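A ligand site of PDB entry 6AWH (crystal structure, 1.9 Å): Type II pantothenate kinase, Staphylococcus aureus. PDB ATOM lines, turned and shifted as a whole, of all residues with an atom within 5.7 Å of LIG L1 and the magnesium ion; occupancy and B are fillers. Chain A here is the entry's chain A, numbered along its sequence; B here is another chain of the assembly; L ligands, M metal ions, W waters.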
ATOM      1  N   ASP A   6      -1.909 -28.164 -10.906  1.00  0.00           N
ATOM      2  CA  ASP A   6      -0.773 -28.016 -11.831  1.00  0.00           C
ATOM      3  C   ASP A   6      -0.673 -26.543 -12.193  1.00  0.00           C
ATOM      4  O   ASP A   6      -1.436 -26.031 -13.019  1.00  0.00           O
ATOM      5  CB  ASP A   6      -0.943 -28.892 -13.060  1.00  0.00           C
ATOM      6  CG  ASP A   6       0.265 -28.903 -13.964  1.00  0.00           C
ATOM      7  OD1 ASP A   6       1.210 -28.091 -13.762  1.00  0.00           O
ATOM      8  OD2 ASP A   6       0.249 -29.708 -14.930  1.00  0.00           O
ATOM      9  N   ALA A   7       0.232 -25.841 -11.516  1.00  0.00           N
ATOM     10  CA  ALA A   7       0.386 -24.380 -11.666  1.00  0.00           C
ATOM     11  C   ALA A   7       1.517 -24.098 -12.644  1.00  0.00           C
ATOM     12  O   ALA A   7       2.688 -24.052 -12.271  1.00  0.00           O
ATOM     13  CB  ALA A   7       0.633 -23.688 -10.325  1.00  0.00           C
ATOM     14  N   GLY A   8       1.136 -23.971 -13.892  1.00  0.00           N
ATOM     15  CA  GLY A   8       2.107 -23.838 -14.974  1.00  0.00           C
ATOM     16  C   GLY A   8       2.440 -22.400 -15.267  1.00  0.00           C
ATOM     17  O   GLY A   8       1.973 -21.460 -14.582  1.00  0.00           O
ATOM     18  N   GLY A   9       3.239 -22.222 -16.303  1.00  0.00           N
ATOM     19  CA  GLY A   9       3.678 -20.874 -16.722  1.00  0.00           C
ATOM     20  C   GLY A   9       2.567 -19.926 -17.151  1.00  0.00           C
ATOM     21  O   GLY A   9       2.669 -18.712 -16.968  1.00  0.00           O
ATOM     22  N   THR A  10       1.492 -20.472 -17.698  1.00  0.00           N
ATOM     23  CA  THR A  10       0.365 -19.657 -18.189  1.00  0.00           C
ATOM     24  C   THR A  10      -0.995 -19.971 -17.515  1.00  0.00           C
ATOM     25  O   THR A  10      -1.762 -19.048 -17.193  1.00  0.00           O
ATOM     26  CB  THR A  10       0.222 -19.777 -19.701  1.00  0.00           C
ATOM     27  OG1 THR A  10       1.469 -19.493 -20.306  1.00  0.00           O
ATOM     28  CG2 THR A  10      -0.801 -18.787 -20.238  1.00  0.00           C
ATOM     29  N   LEU A  11      -1.308 -21.240 -17.364  1.00  0.00           N
ATOM     30  CA  LEU A  11      -2.557 -21.669 -16.726  1.00  0.00           C
ATOM     31  C   LEU A  11      -2.303 -22.518 -15.490  1.00  0.00           C
ATOM     32  O   LEU A  11      -1.361 -23.299 -15.398  1.00  0.00           O
ATOM     33  CB  LEU A  11      -3.436 -22.444 -17.702  1.00  0.00           C
ATOM     34  CG  LEU A  11      -3.778 -21.683 -18.995  1.00  0.00           C
ATOM     35  CD1 LEU A  11      -4.526 -22.594 -19.941  1.00  0.00           C
ATOM     36  CD2 LEU A  11      -4.598 -20.437 -18.713  1.00  0.00           C
ATOM     37  N   ILE A  12      -3.211 -22.346 -14.535  1.00  0.00           N
ATOM     38  CA  ILE A  12      -3.315 -23.165 -13.354  1.00  0.00           C
ATOM     39  C   ILE A  12      -4.472 -24.114 -13.593  1.00  0.00           C
ATOM     40  O   ILE A  12      -5.622 -23.661 -13.778  1.00  0.00           O
ATOM     41  CB  ILE A  12      -3.539 -22.318 -12.075  1.00  0.00           C
ATOM     42  CG1 ILE A  12      -2.346 -21.377 -11.860  1.00  0.00           C
ATOM     43  CG2 ILE A  12      -3.670 -23.208 -10.840  1.00  0.00           C
ATOM     44  CD1 ILE A  12      -2.574 -20.305 -10.826  1.00  0.00           C
ATOM     45  N   LYS A  13      -4.184 -25.412 -13.559  1.00  0.00           N
ATOM     46  CA  LYS A  13      -5.226 -26.455 -13.689  1.00  0.00           C
ATOM     47  C   LYS A  13      -5.503 -27.021 -12.320  1.00  0.00           C
ATOM     48  O   LYS A  13      -4.588 -27.437 -11.623  1.00  0.00           O
ATOM     49  CB  LYS A  13      -4.800 -27.607 -14.619  1.00  0.00           C
ATOM     50  CG  LYS A  13      -4.900 -27.288 -16.108  1.00  0.00           C
ATOM     51  CD  LYS A  13      -3.865 -26.252 -16.568  1.00  0.00           C
ATOM     52  CE  LYS A  13      -2.422 -26.720 -16.314  1.00  0.00           C
ATOM     53  NZ  LYS A  13      -1.430 -25.812 -16.905  1.00  0.00           N
ATOM     54  N   THR A  26      -9.924 -24.302 -14.614  1.00  0.00           N
ATOM     55  CA  THR A  26      -8.800 -23.556 -15.181  1.00  0.00           C
ATOM     56  C   THR A  26      -8.821 -22.111 -14.689  1.00  0.00           C
ATOM     57  O   THR A  26      -9.860 -21.469 -14.674  1.00  0.00           O
ATOM     58  CB  THR A  26      -8.823 -23.551 -16.704  1.00  0.00           C
ATOM     59  OG1 THR A  26      -8.688 -24.892 -17.168  1.00  0.00           O
ATOM     60  CG2 THR A  26      -7.677 -22.724 -17.235  1.00  0.00           C
ATOM     61  N   LEU A  28      -6.106 -18.471 -14.763  1.00  0.00           N
ATOM     62  CA  LEU A  28      -4.897 -17.847 -15.270  1.00  0.00           C
ATOM     63  C   LEU A  28      -3.819 -17.832 -14.193  1.00  0.00           C
ATOM     64  O   LEU A  28      -4.078 -17.516 -13.022  1.00  0.00           O
ATOM     65  CB  LEU A  28      -5.135 -16.426 -15.775  1.00  0.00           C
ATOM     66  CG  LEU A  28      -6.234 -16.245 -16.826  1.00  0.00           C
ATOM     67  CD1 LEU A  28      -6.349 -14.774 -17.182  1.00  0.00           C
ATOM     68  CD2 LEU A  28      -5.976 -17.082 -18.069  1.00  0.00           C
ATOM     69  N   THR A  29      -2.598 -18.156 -14.599  1.00  0.00           N
ATOM     70  CA  THR A  29      -1.453 -18.051 -13.689  1.00  0.00           C
ATOM     71  C   THR A  29      -1.280 -16.600 -13.199  1.00  0.00           C
ATOM     72  O   THR A  29      -0.914 -16.390 -12.040  1.00  0.00           O
ATOM     73  CB  THR A  29      -0.163 -18.612 -14.326  1.00  0.00           C
ATOM     74  OG1 THR A  29      -0.312 -20.027 -14.495  1.00  0.00           O
ATOM     75  CG2 THR A  29       1.051 -18.376 -13.427  1.00  0.00           C
ATOM     76  N   GLY A  52       5.654 -25.253 -12.446  1.00  0.00           N
ATOM     77  CA  GLY A  52       6.616 -24.187 -12.105  1.00  0.00           C
ATOM     78  C   GLY A  52       6.206 -23.231 -10.995  1.00  0.00           C
ATOM     79  O   GLY A  52       7.050 -22.754 -10.230  1.00  0.00           O
ATOM     80  N   GLU A  70       6.583 -32.185 -12.233  1.00  0.00           N
ATOM     81  CA  GLU A  70       5.503 -32.148 -13.247  1.00  0.00           C
ATOM     82  C   GLU A  70       5.550 -33.267 -14.286  1.00  0.00           C
ATOM     83  O   GLU A  70       4.514 -33.698 -14.780  1.00  0.00           O
ATOM     84  CB  GLU A  70       5.400 -30.773 -13.937  1.00  0.00           C
ATOM     85  CG  GLU A  70       6.610 -30.337 -14.757  1.00  0.00           C
ATOM     86  CD  GLU A  70       6.324 -29.056 -15.543  1.00  0.00           C
ATOM     87  OE1 GLU A  70       5.665 -29.151 -16.617  1.00  0.00           O
ATOM     88  OE2 GLU A  70       6.746 -27.973 -15.078  1.00  0.00           O
ATOM     89  N   ASN A  96       3.682 -32.875 -24.278  1.00  0.00           N
ATOM     90  CA  ASN A  96       2.984 -31.904 -23.442  1.00  0.00           C
ATOM     91  C   ASN A  96       3.225 -30.493 -24.014  1.00  0.00           C
ATOM     92  O   ASN A  96       4.278 -29.892 -23.810  1.00  0.00           O
ATOM     93  CB  ASN A  96       3.494 -31.986 -22.014  1.00  0.00           C
ATOM     94  CG  ASN A  96       2.663 -31.201 -21.021  1.00  0.00           C
ATOM     95  OD1 ASN A  96       1.730 -30.509 -21.381  1.00  0.00           O
ATOM     96  ND2 ASN A  96       2.970 -31.367 -19.750  1.00  0.00           N
ATOM     97  N   VAL A  97       2.219 -30.008 -24.725  1.00  0.00           N
ATOM     98  CA  VAL A  97       2.297 -28.723 -25.441  1.00  0.00           C
ATOM     99  C   VAL A  97       1.656 -27.667 -24.539  1.00  0.00           C
ATOM    100  O   VAL A  97       0.466 -27.372 -24.642  1.00  0.00           O
ATOM    101  CB  VAL A  97       1.596 -28.761 -26.803  1.00  0.00           C
ATOM    102  CG1 VAL A  97       1.919 -27.481 -27.588  1.00  0.00           C
ATOM    103  CG2 VAL A  97       2.050 -29.983 -27.598  1.00  0.00           C
ATOM    104  N   GLY A  98       2.477 -27.167 -23.649  1.00  0.00           N
ATOM    105  CA  GLY A  98       2.077 -26.148 -22.663  1.00  0.00           C
ATOM    106  C   GLY A  98       2.526 -24.779 -23.143  1.00  0.00           C
ATOM    107  O   GLY A  98       2.508 -24.508 -24.341  1.00  0.00           O
ATOM    108  N   THR A  99       2.944 -23.924 -22.214  1.00  0.00           N
ATOM    109  CA  THR A  99       3.625 -22.671 -22.547  1.00  0.00           C
ATOM    110  C   THR A  99       4.822 -23.001 -23.450  1.00  0.00           C
ATOM    111  O   THR A  99       5.004 -22.411 -24.515  1.00  0.00           O
ATOM    112  CB  THR A  99       4.048 -21.927 -21.290  1.00  0.00           C
ATOM    113  OG1 THR A  99       2.895 -21.734 -20.446  1.00  0.00           O
ATOM    114  CG2 THR A  99       4.671 -20.562 -21.660  1.00  0.00           C
ATOM    115  N   GLY A 100       5.614 -23.962 -22.991  1.00  0.00           N
ATOM    116  CA  GLY A 100       6.590 -24.658 -23.843  1.00  0.00           C
ATOM    117  C   GLY A 100       6.223 -26.140 -23.977  1.00  0.00           C
ATOM    118  O   GLY A 100       5.283 -26.625 -23.349  1.00  0.00           O
ATOM    119  N   THR A 101       7.017 -26.853 -24.769  1.00  0.00           N
ATOM    120  CA  THR A 101       6.726 -28.219 -25.121  1.00  0.00           C
ATOM    121  C   THR A 101       7.794 -29.175 -24.562  1.00  0.00           C
ATOM    122  O   THR A 101       8.962 -29.006 -24.816  1.00  0.00           O
ATOM    123  CB  THR A 101       6.595 -28.381 -26.640  1.00  0.00           C
ATOM    124  OG1 THR A 101       5.481 -27.597 -27.084  1.00  0.00           O
ATOM    125  CG2 THR A 101       6.380 -29.843 -27.059  1.00  0.00           C
ATOM    126  N   GLY A 120       5.523 -23.814 -28.605  1.00  0.00           N
ATOM    127  CA  GLY A 120       4.309 -24.270 -27.930  1.00  0.00           C
ATOM    128  C   GLY A 120       3.289 -23.132 -27.824  1.00  0.00           C
ATOM    129  O   GLY A 120       3.268 -22.235 -28.658  1.00  0.00           O
ATOM    130  N   GLY A 121       2.422 -23.205 -26.822  1.00  0.00           N
ATOM    131  CA  GLY A 121       1.340 -22.272 -26.618  1.00  0.00           C
ATOM    132  C   GLY A 121       1.809 -20.853 -26.363  1.00  0.00           C
ATOM    133  O   GLY A 121       1.145 -19.885 -26.740  1.00  0.00           O
ATOM    134  N   GLY A 122       2.920 -20.743 -25.656  1.00  0.00           N
ATOM    135  CA  GLY A 122       3.568 -19.451 -25.355  1.00  0.00           C
ATOM    136  C   GLY A 122       3.952 -18.705 -26.615  1.00  0.00           C
ATOM    137  O   GLY A 122       3.730 -17.504 -26.718  1.00  0.00           O
ATOM    138  N   ILE A 124       2.588 -19.304 -29.632  1.00  0.00           N
ATOM    139  CA  ILE A 124       1.336 -18.997 -30.300  1.00  0.00           C
ATOM    140  C   ILE A 124       0.812 -17.627 -29.823  1.00  0.00           C
ATOM    141  O   ILE A 124       0.467 -16.755 -30.607  1.00  0.00           O
ATOM    142  CB  ILE A 124       0.281 -20.114 -30.118  1.00  0.00           C
ATOM    143  CG1 ILE A 124       0.691 -21.331 -30.948  1.00  0.00           C
ATOM    144  CG2 ILE A 124      -1.103 -19.644 -30.531  1.00  0.00           C
ATOM    145  CD1 ILE A 124      -0.078 -22.601 -30.634  1.00  0.00           C
ATOM    146  N   GLN A 125       0.766 -17.454 -28.515  1.00  0.00           N
ATOM    147  CA  GLN A 125       0.306 -16.192 -27.918  1.00  0.00           C
ATOM    148  C   GLN A 125       1.229 -15.004 -28.173  1.00  0.00           C
ATOM    149  O   GLN A 125       0.786 -13.940 -28.557  1.00  0.00           O
ATOM    150  CB  GLN A 125       0.144 -16.350 -26.417  1.00  0.00           C
ATOM    151  CG  GLN A 125      -1.031 -17.245 -26.053  1.00  0.00           C
ATOM    152  CD  GLN A 125      -1.343 -17.150 -24.602  1.00  0.00           C
ATOM    153  OE1 GLN A 125      -2.215 -16.371 -24.183  1.00  0.00           O
ATOM    154  NE2 GLN A 125      -0.629 -17.921 -23.798  1.00  0.00           N
ATOM    155  N   TYR A 137      -6.835 -14.577 -25.827  1.00  0.00           N
ATOM    156  CA  TYR A 137      -6.577 -15.933 -26.354  1.00  0.00           C
ATOM    157  C   TYR A 137      -7.677 -16.453 -27.274  1.00  0.00           C
ATOM    158  O   TYR A 137      -7.418 -16.993 -28.348  1.00  0.00           O
ATOM    159  CB  TYR A 137      -6.332 -16.929 -25.218  1.00  0.00           C
ATOM    160  CG  TYR A 137      -6.123 -18.339 -25.743  1.00  0.00           C
ATOM    161  CD1 TYR A 137      -4.902 -18.709 -26.313  1.00  0.00           C
ATOM    162  CD2 TYR A 137      -7.150 -19.290 -25.689  1.00  0.00           C
ATOM    163  CE1 TYR A 137      -4.710 -19.970 -26.830  1.00  0.00           C
ATOM    164  CE2 TYR A 137      -6.949 -20.590 -26.191  1.00  0.00           C
ATOM    165  CZ  TYR A 137      -5.711 -20.917 -26.749  1.00  0.00           C
ATOM    166  OH  TYR A 137      -5.482 -22.181 -27.246  1.00  0.00           O
ATOM    167  N   GLY A 224      -1.929 -30.900 -23.306  1.00  0.00           N
ATOM    168  CA  GLY A 224      -1.607 -29.505 -23.016  1.00  0.00           C
ATOM    169  C   GLY A 224      -2.758 -28.623 -23.386  1.00  0.00           C
ATOM    170  O   GLY A 224      -3.559 -28.998 -24.244  1.00  0.00           O
ATOM    171  N   SER A 225      -2.872 -27.474 -22.718  1.00  0.00           N
ATOM    172  CA  SER A 225      -3.975 -26.565 -22.963  1.00  0.00           C
ATOM    173  C   SER A 225      -3.858 -25.832 -24.316  1.00  0.00           C
ATOM    174  O   SER A 225      -4.825 -25.235 -24.753  1.00  0.00           O
ATOM    175  CB  SER A 225      -4.154 -25.565 -21.848  1.00  0.00           C
ATOM    176  OG  SER A 225      -4.143 -26.187 -20.603  1.00  0.00           O
ATOM    177  N   SER A 226      -2.708 -25.939 -24.987  1.00  0.00           N
ATOM    178  CA  SER A 226      -2.503 -25.323 -26.306  1.00  0.00           C
ATOM    179  C   SER A 226      -3.479 -25.837 -27.351  1.00  0.00           C
ATOM    180  O   SER A 226      -3.686 -25.178 -28.356  1.00  0.00           O
ATOM    181  CB  SER A 226      -1.071 -25.527 -26.832  1.00  0.00           C
ATOM    182  OG  SER A 226      -0.138 -24.982 -25.950  1.00  0.00           O
ATOM    183  N   PHE A 227      -4.032 -27.024 -27.120  1.00  0.00           N
ATOM    184  CA  PHE A 227      -5.041 -27.603 -27.972  1.00  0.00           C
ATOM    185  C   PHE A 227      -6.484 -27.118 -27.716  1.00  0.00           C
ATOM    186  O   PHE A 227      -7.355 -27.351 -28.548  1.00  0.00           O
ATOM    187  CB  PHE A 227      -4.962 -29.121 -27.919  1.00  0.00           C
ATOM    188  CG  PHE A 227      -3.673 -29.669 -28.443  1.00  0.00           C
ATOM    189  CD1 PHE A 227      -3.402 -29.650 -29.795  1.00  0.00           C
ATOM    190  CD2 PHE A 227      -2.697 -30.141 -27.565  1.00  0.00           C
ATOM    191  CE1 PHE A 227      -2.214 -30.149 -30.274  1.00  0.00           C
ATOM    192  CE2 PHE A 227      -1.500 -30.604 -28.042  1.00  0.00           C
ATOM    193  CZ  PHE A 227      -1.258 -30.630 -29.394  1.00  0.00           C
ATOM    194  N   HIS A 228      -6.721 -26.414 -26.624  1.00  0.00           N
ATOM    195  CA  HIS A 228      -8.059 -25.840 -26.345  1.00  0.00           C
ATOM    196  C   HIS A 228      -8.418 -24.687 -27.268  1.00  0.00           C
ATOM    197  O   HIS A 228      -7.660 -23.713 -27.415  1.00  0.00           O
ATOM    198  CB  HIS A 228      -8.170 -25.302 -24.902  1.00  0.00           C
ATOM    199  CG  HIS A 228      -7.976 -26.327 -23.817  1.00  0.00           C
ATOM    200  ND1 HIS A 228      -7.623 -27.656 -24.028  1.00  0.00           N
ATOM    201  CD2 HIS A 228      -8.028 -26.178 -22.471  1.00  0.00           C
ATOM    202  CE1 HIS A 228      -7.536 -28.277 -22.866  1.00  0.00           C
ATOM    203  NE2 HIS A 228      -7.766 -27.394 -21.902  1.00  0.00           N
ATOM    204  N   ALA A 255      -5.210 -31.866 -20.697  1.00  0.00           N
ATOM    205  CA  ALA A 255      -4.532 -30.679 -20.091  1.00  0.00           C
ATOM    206  C   ALA A 255      -4.425 -30.729 -18.571  1.00  0.00           C
ATOM    207  O   ALA A 255      -3.616 -30.021 -17.990  1.00  0.00           O
ATOM    208  CB  ALA A 255      -5.216 -29.390 -20.525  1.00  0.00           C
ATOM    209  N   ILE B 159       9.479 -19.475 -15.418  1.00  0.00           N
ATOM    210  CA  ILE B 159       8.324 -20.317 -15.061  1.00  0.00           C
ATOM    211  C   ILE B 159       8.461 -20.853 -13.629  1.00  0.00           C
ATOM    212  O   ILE B 159       7.509 -20.805 -12.856  1.00  0.00           O
ATOM    213  CB  ILE B 159       8.121 -21.483 -16.058  1.00  0.00           C
ATOM    214  CG1 ILE B 159       7.726 -20.914 -17.417  1.00  0.00           C
ATOM    215  CG2 ILE B 159       7.076 -22.487 -15.549  1.00  0.00           C
ATOM    216  CD1 ILE B 159       7.539 -21.918 -18.530  1.00  0.00           C
HETATM  217  P1  LIG L   1       4.188 -24.981 -18.864  1.00  0.00           P
HETATM  218  O1  LIG L   1       3.791 -26.426 -18.664  1.00  0.00           O
HETATM  219  O2  LIG L   1       4.626 -24.327 -17.558  1.00  0.00           O
HETATM  220  O3  LIG L   1       5.049 -24.761 -20.085  1.00  0.00           O
HETATM  221  P2  LIG L   1       1.271 -24.429 -18.787  1.00  0.00           P
HETATM  222  O4  LIG L   1       0.691 -23.134 -18.211  1.00  0.00           O
HETATM  223  O5  LIG L   1       1.200 -25.649 -17.894  1.00  0.00           O
HETATM  224  O6  LIG L   1       2.784 -24.210 -19.272  1.00  0.00           O
HETATM  225  P3  LIG L   1      -0.802 -25.346 -20.623  1.00  0.00           P
HETATM  226  O7  LIG L   1      -1.765 -24.832 -19.587  1.00  0.00           O
HETATM  227  O8  LIG L   1      -0.755 -26.789 -20.977  1.00  0.00           O
HETATM  228  O9  LIG L   1       0.675 -24.807 -20.221  1.00  0.00           O
HETATM  229  O10 LIG L   1      -0.969 -24.550 -21.988  1.00  0.00           O
HETATM  230  C1  LIG L   1      -0.905 -23.118 -22.028  1.00  0.00           C
HETATM  231  C2  LIG L   1      -1.312 -22.652 -23.419  1.00  0.00           C
HETATM  232  O11 LIG L   1      -2.675 -23.022 -23.690  1.00  0.00           O
HETATM  233  C3  LIG L   1      -1.277 -21.139 -23.651  1.00  0.00           C
HETATM  234  O12 LIG L   1       0.042 -20.720 -23.942  1.00  0.00           O
HETATM  235  C4  LIG L   1      -2.246 -20.972 -24.801  1.00  0.00           C
HETATM  236  O13 LIG L   1      -1.636 -21.351 -26.043  1.00  0.00           O
HETATM  237  C5  LIG L   1      -3.321 -22.040 -24.509  1.00  0.00           C
HETATM  238  N1  LIG L   1      -4.542 -21.565 -23.791  1.00  0.00           N
HETATM  239  C6  LIG L   1      -5.682 -22.275 -23.711  1.00  0.00           C
HETATM  240  N2  LIG L   1      -6.622 -21.635 -22.996  1.00  0.00           N
HETATM  241  C7  LIG L   1      -6.094 -20.481 -22.628  1.00  0.00           C
HETATM  242  C8  LIG L   1      -6.571 -19.334 -21.862  1.00  0.00           C
HETATM  243  N3  LIG L   1      -7.826 -19.370 -21.373  1.00  0.00           N
HETATM  244  N4  LIG L   1      -5.727 -18.315 -21.646  1.00  0.00           N
HETATM  245  C9  LIG L   1      -4.484 -18.304 -22.121  1.00  0.00           C
HETATM  246  N5  LIG L   1      -3.998 -19.329 -22.844  1.00  0.00           N
HETATM  247  C10 LIG L   1      -4.727 -20.421 -23.122  1.00  0.00           C
HETATM  248  C1  LG2 L   2       7.537 -26.012 -18.033  1.00  0.00           C
HETATM  249  C2  LG2 L   2       8.684 -26.519 -18.903  1.00  0.00           C
HETATM  250  C3  LG2 L   2       9.088 -27.930 -18.360  1.00  0.00           C
HETATM  251  C4  LG2 L   2       9.866 -25.554 -18.803  1.00  0.00           C
HETATM  252  C5  LG2 L   2       8.157 -26.608 -20.379  1.00  0.00           C
HETATM  253  O1  LG2 L   2       7.619 -25.309 -20.778  1.00  0.00           O
HETATM  254  C6  LG2 L   2       9.233 -27.049 -21.378  1.00  0.00           C
HETATM  255  O2  LG2 L   2       9.624 -28.207 -21.428  1.00  0.00           O
HETATM  256  N1  LG2 L   2       9.719 -26.080 -22.219  1.00  0.00           N
HETATM  257  C7  LG2 L   2      10.768 -26.358 -23.209  1.00  0.00           C
HETATM  258  C8  LG2 L   2      12.139 -26.471 -22.500  1.00  0.00           C
HETATM  259  C9  LG2 L   2      13.159 -27.042 -23.449  1.00  0.00           C
HETATM  260  O3  LG2 L   2      13.372 -28.244 -23.517  1.00  0.00           O
HETATM  261  N2  LG2 L   2      13.806 -26.166 -24.209  1.00  0.00           N
HETATM  262  C10 LG2 L   2      14.818 -26.601 -25.190  1.00  0.00           C
HETATM  263  C11 LG2 L   2      15.259 -25.389 -25.992  1.00  0.00           C
HETATM  264  C12 LG2 L   2      16.646 -25.034 -25.572  1.00  0.00           C
HETATM  265  C13 LG2 L   2      17.024 -23.746 -26.207  1.00  0.00           C
HETATM  266  C14 LG2 L   2      18.341 -23.278 -25.694  1.00  0.00           C
HETATM  267  O4  LG2 L   2      18.060 -22.452 -24.547  1.00  0.00           O
HETATM  268  C15 LG2 L   2      19.208 -21.719 -24.107  1.00  0.00           C
HETATM  269 MG    MG M   1       2.169 -27.373 -17.954  1.00  0.00          MG
HETATM  270  O   HOH W   1       3.259 -29.228 -17.869  1.00  0.00           O
HETATM  271  O   HOH W   2       0.385 -28.338 -17.181  1.00  0.00           O
HETATM  272  O   HOH W   3       5.103 -25.728 -15.201  1.00  0.00           O
HETATM  273  O   HOH W   4       2.676 -27.245 -15.805  1.00  0.00           O
HETATM  274  O   HOH W   5       1.548 -27.815 -19.921  1.00  0.00           O
HETATM  275  O   HOH W   6      -1.567 -28.617 -19.010  1.00  0.00           O
HETATM  276  O   HOH W   7      -6.411 -15.684 -20.947  1.00  0.00           O
HETATM  277  O   HOH W   8       4.688 -28.090 -20.728  1.00  0.00           O
HETATM  278  O   HOH W   9      -8.060 -23.455 -21.339  1.00  0.00           O
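The backbone NH (N) of Thr 99 lies within hydrogen-bond range of an oxygen (O6) of LIG L1 (3.0 Å).
An oxygen (O6) of LIG L1 lies within hydrogen-bond range of the side-chain hydroxyl (OG1) of Thr 99.
An oxygen (O7) of LIG L1 is in salt-bridge range of the side-chain amino group (NZ) of Lys 13 (2.9 Å).
The backbone NH (N) of Gly 9 is in hydrogen-bond range of an oxygen (O2) of LIG L1 (2.8 Å).
O8 of LIG L1 lies within hydrogen-bond range of N of Ser 225.
OG of Ser 225 is in hydrogen-bond range of O7 of LIG L1 (2.9 Å).
O4 of LIG L1 sits at hydrogen-bond distance from N of Thr 10, 2.8 Å away.
N of Leu 11 sits at hydrogen-bond distance from O4 of LIG L1.
NE2 of Gln 125 sits at hydrogen-bond distance from O12 of LIG L1, at 2.9 Å.
O12 of LIG L1 lies close to O of Gly 121, at 3.1 Å.
N of Gly 100 lies within hydrogen-bond range of O3 of LIG L1 (3.1 Å).
N of Ser 226 is in hydrogen-bond range of O11 of LIG L1 (3.2 Å).
An oxygen (O12) of LIG L1 sits at hydrogen-bond distance from the backbone NH (N) of Gly 122, 3.3 Å away.
An oxygen (O1) of LG2 L2 sits at hydrogen-bond distance from the backbone NH (N) of Gly 100 (3.3 Å).
No residue comes within 4 Å of the magnesium ion.
The nearest printed residue that does not touch the magnesium ion is Lys 13 (4.1 Å).
Water W2 lies within hydrogen-bond range of OD2 of Asp 6 (2.6 Å) and NZ of Lys 13 (3.1 Å).
Water W5 bridges an oxygen (O8) of LIG L1 and the side-chain amide oxygen of Asn 96.
Water W1 lies within hydrogen-bond range of the side-chain carboxylate of Glu 70 (2.7 Å) and the side-chain amide nitrogen of Asn 96 (2.9 Å).
Water W3 lies within hydrogen-bond range of an oxygen (O2) of LIG L1 (2.8 Å), the side-chain carboxylate (OE2) of Glu 70 (2.8 Å) and the backbone NH (N) of Gly 52 (2.8 Å).
Water W8 lies within hydrogen-bond range of O of Gly 100 and O3 of LIG L1.
Water W6 lies within hydrogen-bond range of the backbone carbonyl oxygen of Ala 255 and an oxygen (O8) of LIG L1.
The magnesium ion is bound by O5 of LIG L1 (2.0 Å), O1 of LIG L1 (2.0 Å), water W5 (2.1 Å), water W1 (2.2 Å), water W2 (2.2 Å) and water W4 (2.2 Å).
The magnesium ion has six donor atoms within binding distance.
C of Gly 8 touches O4 of LIG L1, at 3.5 Å.
Leu 28 touches LIG L1.
Glu 70 touches LIG L1 (OE1 to O1, 3.9 Å).
Val 97 touches LIG L1 (O to O8, 3.9 Å).
Gly 98 touches LIG L1.
CZ of Tyr 137 touches N1 of LIG L1 (3.2 Å).
CA of Gly 224 touches O8 of LIG L1 (3.5 Å).
Ile 159 of chain B touches LIG L1.
Hydrophobic or aromatic side chains that line LIG L1: Leu 11, Leu 28, Tyr 137 and Ile 159 of chain B.
Within 4 Å of LIG L1: Gly 8, Gly 9, Thr 10, Leu 11, Lys 13, Leu 28, Glu 70, Val 97, Gly 98, Thr 99, Gly 100, Gly 121, Gly 122, Gln 125, Tyr 137, Gly 224, Ser 225, Ser 226 and Ile 159 of chain B.
The nearest printed residue that does not touch LIG L1 is His 228 (4.1 Å).
OG1 of Thr 99 lies within hydrogen-bond range of OG1 of Thr 10 (2.7 Å).
The side-chain amino group (NZ) of Lys 13 is in hydrogen-bond range of the backbone carbonyl oxygen (O) of Leu 11 (2.9 Å).
The backbone carbonyl oxygen (O) of Lys 13 is in hydrogen-bond range of the backbone NH (N) of Asp 6, 2.9 Å away.
The backbone carbonyl oxygen of Thr 10 sits at hydrogen-bond distance from the backbone NH of Thr 29 (2.9 Å).
The backbone NH (N) of Leu 11 sits at hydrogen-bond distance from the side-chain hydroxyl (OG1) of Thr 29.
OG of Ser 226 is in hydrogen-bond range of O of Gly 98.
O of Val 97 is in hydrogen-bond range of OG of Ser 226 (2.8 Å).
The side-chain hydroxyl (OH) of Tyr 137 lies within hydrogen-bond range of the backbone carbonyl oxygen (O) of His 228 (2.7 Å).
O3 of LIG L1 sits at hydrogen-bond distance from O1 of LG2 L2 (2.7 Å).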
